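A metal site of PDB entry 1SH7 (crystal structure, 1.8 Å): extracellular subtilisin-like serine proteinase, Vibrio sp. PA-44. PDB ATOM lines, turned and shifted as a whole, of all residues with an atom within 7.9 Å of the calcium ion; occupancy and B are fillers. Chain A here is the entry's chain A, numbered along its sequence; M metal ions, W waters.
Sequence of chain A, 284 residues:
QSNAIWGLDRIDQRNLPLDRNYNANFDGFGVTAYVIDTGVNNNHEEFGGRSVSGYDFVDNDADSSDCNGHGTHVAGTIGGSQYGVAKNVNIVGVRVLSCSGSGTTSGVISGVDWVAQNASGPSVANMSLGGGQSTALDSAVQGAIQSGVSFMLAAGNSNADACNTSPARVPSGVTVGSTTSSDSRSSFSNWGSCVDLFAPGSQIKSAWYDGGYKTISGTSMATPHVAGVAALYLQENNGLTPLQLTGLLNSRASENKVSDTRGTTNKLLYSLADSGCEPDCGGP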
ATOM      1  N   GLN A   1      -5.684  -4.593 -17.384  1.00  0.00           N
ATOM      2  CA  GLN A   1      -5.274  -5.269 -16.105  1.00  0.00           C
ATOM      3  C   GLN A   1      -6.184  -4.861 -14.935  1.00  0.00           C
ATOM      4  O   GLN A   1      -7.105  -5.580 -14.601  1.00  0.00           O
ATOM      5  CB  GLN A   1      -3.798  -4.984 -15.793  1.00  0.00           C
ATOM      6  CG  GLN A   1      -2.812  -6.137 -16.147  1.00  0.00           C
ATOM      7  CD  GLN A   1      -1.511  -5.634 -16.788  1.00  0.00           C
ATOM      8  OE1 GLN A   1      -1.539  -4.904 -17.779  1.00  0.00           O
ATOM      9  NE2 GLN A   1      -0.374  -6.041 -16.220  1.00  0.00           N
ATOM     10  N   ALA A   4     -10.150  -2.021 -15.100  1.00  0.00           N
ATOM     11  CA  ALA A   4     -10.682  -2.648 -16.287  1.00  0.00           C
ATOM     12  C   ALA A   4     -12.105  -2.183 -16.506  1.00  0.00           C
ATOM     13  O   ALA A   4     -12.838  -1.958 -15.560  1.00  0.00           O
ATOM     14  CB  ALA A   4     -10.628  -4.178 -16.191  1.00  0.00           C
ATOM     15  N   ILE A   5     -12.463  -1.985 -17.759  1.00  0.00           N
ATOM     16  CA  ILE A   5     -13.818  -1.626 -18.124  1.00  0.00           C
ATOM     17  C   ILE A   5     -14.680  -2.846 -17.912  1.00  0.00           C
ATOM     18  O   ILE A   5     -14.169  -3.981 -17.820  1.00  0.00           O
ATOM     19  CB  ILE A   5     -13.920  -1.086 -19.570  1.00  0.00           C
ATOM     20  CG1 ILE A   5     -13.316  -2.059 -20.573  1.00  0.00           C
ATOM     21  CG2 ILE A   5     -13.246   0.291 -19.677  1.00  0.00           C
ATOM     22  CD1 ILE A   5     -13.644  -1.706 -22.020  1.00  0.00           C
ATOM     23  N   TRP A   6     -15.980  -2.619 -17.794  1.00  0.00           N
ATOM     24  CA  TRP A   6     -16.838  -3.638 -17.161  1.00  0.00           C
ATOM     25  C   TRP A   6     -16.991  -4.929 -17.937  1.00  0.00           C
ATOM     26  O   TRP A   6     -17.129  -5.975 -17.339  1.00  0.00           O
ATOM     27  CB  TRP A   6     -18.238  -3.091 -16.845  1.00  0.00           C
ATOM     28  CG  TRP A   6     -19.195  -3.139 -17.991  1.00  0.00           C
ATOM     29  CD1 TRP A   6     -19.517  -2.119 -18.877  1.00  0.00           C
ATOM     30  CD2 TRP A   6     -20.050  -4.236 -18.329  1.00  0.00           C
ATOM     31  NE1 TRP A   6     -20.467  -2.550 -19.771  1.00  0.00           N
ATOM     32  CE2 TRP A   6     -20.829  -3.843 -19.459  1.00  0.00           C
ATOM     33  CE3 TRP A   6     -20.209  -5.539 -17.840  1.00  0.00           C
ATOM     34  CZ2 TRP A   6     -21.778  -4.687 -20.062  1.00  0.00           C
ATOM     35  CZ3 TRP A   6     -21.128  -6.369 -18.429  1.00  0.00           C
ATOM     36  CH2 TRP A   6     -21.909  -5.938 -19.535  1.00  0.00           C
ATOM     37  N   GLY A   7     -17.001  -4.863 -19.258  1.00  0.00           N
ATOM     38  CA  GLY A   7     -17.176  -6.051 -20.106  1.00  0.00           C
ATOM     39  C   GLY A   7     -16.058  -7.045 -19.917  1.00  0.00           C
ATOM     40  O   GLY A   7     -16.268  -8.249 -19.671  1.00  0.00           O
ATOM     41  N   LEU A   8     -14.832  -6.520 -19.962  1.00  0.00           N
ATOM     42  CA  LEU A   8     -13.660  -7.333 -19.705  1.00  0.00           C
ATOM     43  C   LEU A   8     -13.672  -7.852 -18.269  1.00  0.00           C
ATOM     44  O   LEU A   8     -13.403  -9.030 -18.008  1.00  0.00           O
ATOM     45  CB  LEU A   8     -12.378  -6.516 -19.946  1.00  0.00           C
ATOM     46  CG  LEU A   8     -12.122  -5.909 -21.319  1.00  0.00           C
ATOM     47  CD1 LEU A   8     -10.775  -5.216 -21.285  1.00  0.00           C
ATOM     48  CD2 LEU A   8     -12.220  -6.963 -22.423  1.00  0.00           C
ATOM     49  N   ASP A   9     -14.010  -6.952 -17.345  1.00  0.00           N
ATOM     50  CA  ASP A   9     -14.118  -7.245 -15.928  1.00  0.00           C
ATOM     51  C   ASP A   9     -15.082  -8.403 -15.671  1.00  0.00           C
ATOM     52  O   ASP A   9     -14.802  -9.301 -14.863  1.00  0.00           O
ATOM     53  CB  ASP A   9     -14.614  -5.992 -15.194  1.00  0.00           C
ATOM     54  CG  ASP A   9     -14.571  -6.133 -13.683  1.00  0.00           C
ATOM     55  OD1 ASP A   9     -14.903  -5.120 -13.001  1.00  0.00           O
ATOM     56  OD2 ASP A   9     -14.226  -7.178 -13.092  1.00  0.00           O
ATOM     57  N   ARG A  10     -16.218  -8.400 -16.359  1.00  0.00           N
ATOM     58  CA  ARG A  10     -17.223  -9.436 -16.181  1.00  0.00           C
ATOM     59  C   ARG A  10     -16.830 -10.853 -16.644  1.00  0.00           C
ATOM     60  O   ARG A  10     -17.267 -11.822 -16.053  1.00  0.00           O
ATOM     61  CB  ARG A  10     -18.501  -9.072 -16.926  1.00  0.00           C
ATOM     62  CG  ARG A  10     -19.704  -9.909 -16.568  1.00  0.00           C
ATOM     63  CD  ARG A  10     -20.134  -9.832 -15.109  1.00  0.00           C
ATOM     64  NE  ARG A  10     -21.131 -10.831 -14.704  1.00  0.00           N
ATOM     65  CZ  ARG A  10     -20.863 -12.087 -14.307  1.00  0.00           C
ATOM     66  NH1 ARG A  10     -21.868 -12.870 -13.932  1.00  0.00           N
ATOM     67  NH2 ARG A  10     -19.625 -12.557 -14.246  1.00  0.00           N
ATOM     68  N   ILE A  11     -16.059 -10.978 -17.713  1.00  0.00           N
ATOM     69  CA  ILE A  11     -15.966 -12.255 -18.404  1.00  0.00           C
ATOM     70  C   ILE A  11     -14.915 -13.163 -17.787  1.00  0.00           C
ATOM     71  O   ILE A  11     -14.902 -14.325 -18.127  1.00  0.00           O
ATOM     72  CB  ILE A  11     -15.713 -12.072 -19.936  1.00  0.00           C
ATOM     73  CG1 ILE A  11     -14.335 -11.469 -20.177  1.00  0.00           C
ATOM     74  CG2 ILE A  11     -16.851 -11.269 -20.581  1.00  0.00           C
ATOM     75  CD1 ILE A  11     -13.976 -11.384 -21.595  1.00  0.00           C
ATOM     76  N   ASP A  12     -14.063 -12.652 -16.891  1.00  0.00           N
ATOM     77  CA  ASP A  12     -13.084 -13.473 -16.167  1.00  0.00           C
ATOM     78  C   ASP A  12     -13.537 -13.944 -14.773  1.00  0.00           C
ATOM     79  O   ASP A  12     -12.699 -14.346 -13.961  1.00  0.00           O
ATOM     80  CB  ASP A  12     -11.750 -12.726 -16.017  1.00  0.00           C
ATOM     81  CG  ASP A  12     -11.798 -11.663 -14.922  1.00  0.00           C
ATOM     82  OD1 ASP A  12     -10.728 -11.262 -14.417  1.00  0.00           O
ATOM     83  OD2 ASP A  12     -12.865 -11.181 -14.496  1.00  0.00           O
ATOM     84  N   GLN A  13     -14.847 -13.887 -14.498  1.00  0.00           N
ATOM     85  CA  GLN A  13     -15.416 -14.263 -13.204  1.00  0.00           C
ATOM     86  C   GLN A  13     -16.842 -14.757 -13.365  1.00  0.00           C
ATOM     87  O   GLN A  13     -17.542 -14.422 -14.344  1.00  0.00           O
ATOM     88  CB  GLN A  13     -15.329 -13.096 -12.195  1.00  0.00           C
ATOM     89  CG  GLN A  13     -16.042 -11.822 -12.654  1.00  0.00           C
ATOM     90  CD  GLN A  13     -15.860 -10.714 -11.640  1.00  0.00           C
ATOM     91  OE1 GLN A  13     -14.840 -10.018 -11.683  1.00  0.00           O
ATOM     92  NE2 GLN A  13     -16.794 -10.582 -10.700  1.00  0.00           N
ATOM     93  N   ARG A  14     -17.243 -15.588 -12.413  1.00  0.00           N
ATOM     94  CA  ARG A  14     -18.526 -16.261 -12.446  1.00  0.00           C
ATOM     95  C   ARG A  14     -19.657 -15.353 -12.001  1.00  0.00           C
ATOM     96  O   ARG A  14     -20.692 -15.300 -12.628  1.00  0.00           O
ATOM     97  CB  ARG A  14     -18.447 -17.506 -11.544  1.00  0.00           C
ATOM     98  CG  ARG A  14     -17.494 -18.591 -12.056  1.00  0.00           C
ATOM     99  CD  ARG A  14     -17.870 -19.094 -13.415  1.00  0.00           C
ATOM    100  NE  ARG A  14     -17.018 -20.218 -13.858  1.00  0.00           N
ATOM    101  CZ  ARG A  14     -17.046 -20.679 -15.101  1.00  0.00           C
ATOM    102  NH1 ARG A  14     -17.846 -20.138 -15.989  1.00  0.00           N
ATOM    103  NH2 ARG A  14     -16.266 -21.708 -15.468  1.00  0.00           N
ATOM    104  N   ASN A  15     -19.461 -14.624 -10.899  1.00  0.00           N
ATOM    105  CA  ASN A  15     -20.559 -13.950 -10.222  1.00  0.00           C
ATOM    106  C   ASN A  15     -20.308 -12.464 -10.039  1.00  0.00           C
ATOM    107  O   ASN A  15     -19.187 -12.017 -10.003  1.00  0.00           O
ATOM    108  CB  ASN A  15     -20.797 -14.576  -8.842  1.00  0.00           C
ATOM    109  CG  ASN A  15     -21.493 -15.904  -8.915  1.00  0.00           C
ATOM    110  OD1 ASN A  15     -22.562 -16.055  -9.535  1.00  0.00           O
ATOM    111  ND2 ASN A  15     -20.876 -16.889  -8.317  1.00  0.00           N
ATOM    112  N   PRO A  17     -20.292  -9.368  -7.319  1.00  0.00           N
ATOM    113  CA  PRO A  17     -19.952  -8.089  -7.970  1.00  0.00           C
ATOM    114  C   PRO A  17     -18.690  -8.116  -8.822  1.00  0.00           C
ATOM    115  O   PRO A  17     -17.833  -8.986  -8.644  1.00  0.00           O
ATOM    116  CB  PRO A  17     -19.709  -7.176  -6.749  1.00  0.00           C
ATOM    117  CG  PRO A  17     -19.127  -8.069  -5.736  1.00  0.00           C
ATOM    118  CD  PRO A  17     -19.873  -9.389  -5.899  1.00  0.00           C
ATOM    119  N   LEU A  18     -18.576  -7.135  -9.730  1.00  0.00           N
ATOM    120  CA  LEU A  18     -17.340  -6.868 -10.474  1.00  0.00           C
ATOM    121  C   LEU A  18     -16.186  -6.522  -9.543  1.00  0.00           C
ATOM    122  O   LEU A  18     -16.399  -5.990  -8.463  1.00  0.00           O
ATOM    123  CB  LEU A  18     -17.570  -5.709 -11.439  1.00  0.00           C
ATOM    124  CG  LEU A  18     -18.671  -5.860 -12.470  1.00  0.00           C
ATOM    125  CD1 LEU A  18     -18.851  -4.514 -13.212  1.00  0.00           C
ATOM    126  CD2 LEU A  18     -18.324  -7.011 -13.457  1.00  0.00           C
ATOM    127  N   ASP A  19     -14.961  -6.855  -9.926  1.00  0.00           N
ATOM    128  CA  ASP A  19     -13.791  -6.562  -9.088  1.00  0.00           C
ATOM    129  C   ASP A  19     -12.795  -5.589  -9.708  1.00  0.00           C
ATOM    130  O   ASP A  19     -11.690  -5.391  -9.181  1.00  0.00           O
ATOM    131  CB  ASP A  19     -13.055  -7.855  -8.680  1.00  0.00           C
ATOM    132  CG  ASP A  19     -12.351  -8.504  -9.855  1.00  0.00           C
ATOM    133  OD1 ASP A  19     -11.619  -9.498  -9.636  1.00  0.00           O
ATOM    134  OD2 ASP A  19     -12.475  -8.087 -11.042  1.00  0.00           O
ATOM    135  N   ARG A  20     -13.207  -4.965 -10.808  1.00  0.00           N
ATOM    136  CA  ARG A  20     -12.404  -4.013 -11.552  1.00  0.00           C
ATOM    137  C   ARG A  20     -11.109  -4.590 -12.151  1.00  0.00           C
ATOM    138  O   ARG A  20     -10.181  -3.872 -12.454  1.00  0.00           O
ATOM    139  CB  ARG A  20     -12.148  -2.791 -10.685  1.00  0.00           C
ATOM    140  CG  ARG A  20     -13.459  -2.086 -10.291  1.00  0.00           C
ATOM    141  CD  ARG A  20     -13.216  -0.830  -9.487  1.00  0.00           C
ATOM    142  NE  ARG A  20     -12.756  -1.152  -8.127  1.00  0.00           N
ATOM    143  CZ  ARG A  20     -11.586  -0.770  -7.606  1.00  0.00           C
ATOM    144  NH1 ARG A  20     -11.283  -1.135  -6.358  1.00  0.00           N
ATOM    145  NH2 ARG A  20     -10.720  -0.050  -8.317  1.00  0.00           N
ATOM    146  N   ASN A  21     -11.068  -5.898 -12.309  1.00  0.00           N
ATOM    147  CA  ASN A  21      -9.888  -6.581 -12.797  1.00  0.00           C
ATOM    148  C   ASN A  21     -10.275  -7.457 -13.961  1.00  0.00           C
ATOM    149  O   ASN A  21     -11.355  -8.073 -13.933  1.00  0.00           O
ATOM    150  CB  ASN A  21      -9.255  -7.453 -11.697  1.00  0.00           C
ATOM    151  CG  ASN A  21      -8.348  -6.645 -10.752  1.00  0.00           C
ATOM    152  OD1 ASN A  21      -7.197  -6.375 -11.053  1.00  0.00           O
ATOM    153  ND2 ASN A  21      -8.893  -6.259  -9.622  1.00  0.00           N
ATOM    154  N   TYR A  22      -9.428  -7.493 -14.991  1.00  0.00           N
ATOM    155  CA  TYR A  22      -9.526  -8.495 -16.067  1.00  0.00           C
ATOM    156  C   TYR A  22      -8.210  -9.305 -16.049  1.00  0.00           C
ATOM    157  O   TYR A  22      -7.147  -8.807 -16.384  1.00  0.00           O
ATOM    158  CB  TYR A  22      -9.768  -7.843 -17.434  1.00  0.00           C
ATOM    159  CG  TYR A  22      -9.695  -8.827 -18.595  1.00  0.00           C
ATOM    160  CD1 TYR A  22     -10.536  -9.914 -18.660  1.00  0.00           C
ATOM    161  CD2 TYR A  22      -8.730  -8.685 -19.587  1.00  0.00           C
ATOM    162  CE1 TYR A  22     -10.432 -10.843 -19.680  1.00  0.00           C
ATOM    163  CE2 TYR A  22      -8.661  -9.543 -20.602  1.00  0.00           C
ATOM    164  CZ  TYR A  22      -9.501 -10.654 -20.630  1.00  0.00           C
ATOM    165  OH  TYR A  22      -9.361 -11.538 -21.675  1.00  0.00           O
ATOM    166  N   ASN A  23      -8.334 -10.560 -15.653  1.00  0.00           N
ATOM    167  CA  ASN A  23      -7.225 -11.486 -15.553  1.00  0.00           C
ATOM    168  C   ASN A  23      -7.236 -12.335 -16.816  1.00  0.00           C
ATOM    169  O   ASN A  23      -8.282 -12.699 -17.309  1.00  0.00           O
ATOM    170  CB  ASN A  23      -7.404 -12.431 -14.374  1.00  0.00           C
ATOM    171  CG  ASN A  23      -7.340 -11.730 -13.023  1.00  0.00           C
ATOM    172  OD1 ASN A  23      -8.231 -11.900 -12.201  1.00  0.00           O
ATOM    173  ND2 ASN A  23      -6.267 -11.021 -12.775  1.00  0.00           N
HETATM  174 CA    CA M   1     -13.135  -9.355 -13.047  1.00  0.00          CA
HETATM  175  O   HOH W   1     -11.810 -10.764 -11.790  1.00  0.00           O
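OD1 of Asp 12 sits at hydrogen-bond distance from N of Asn 23, 2.8 Å away.
The backbone NH of Arg 20 lies within hydrogen-bond range of the side-chain carboxylate of Asp 9.
O of Pro 17 sits at hydrogen-bond distance from NE2 of Gln 13, 2.8 Å away.
The side-chain amide nitrogen (NE2) of Gln 13 sits at hydrogen-bond distance from the backbone carbonyl oxygen (O) of Asn 15 (2.9 Å).
The backbone carbonyl oxygen of Gln 13 is in hydrogen-bond range of the guanidinium group of Arg 10, at 2.8 Å.
The calcium ion is bound by the side-chain amide oxygen of Gln 13, water W1, the side-chain carboxylate of Asp 12, the backbone carbonyl oxygen of Asn 21, the side-chain carboxylate of Asp 9, the side-chain carboxylate of Asp 19 and the backbone carbonyl oxygen of Asp 9.
The calcium ion has seven donor atoms within binding distance.
Water W1 lies within hydrogen-bond range of OD1 of Asp 19 (2.5 Å) and OD1 of Asp 12 (2.9 Å).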
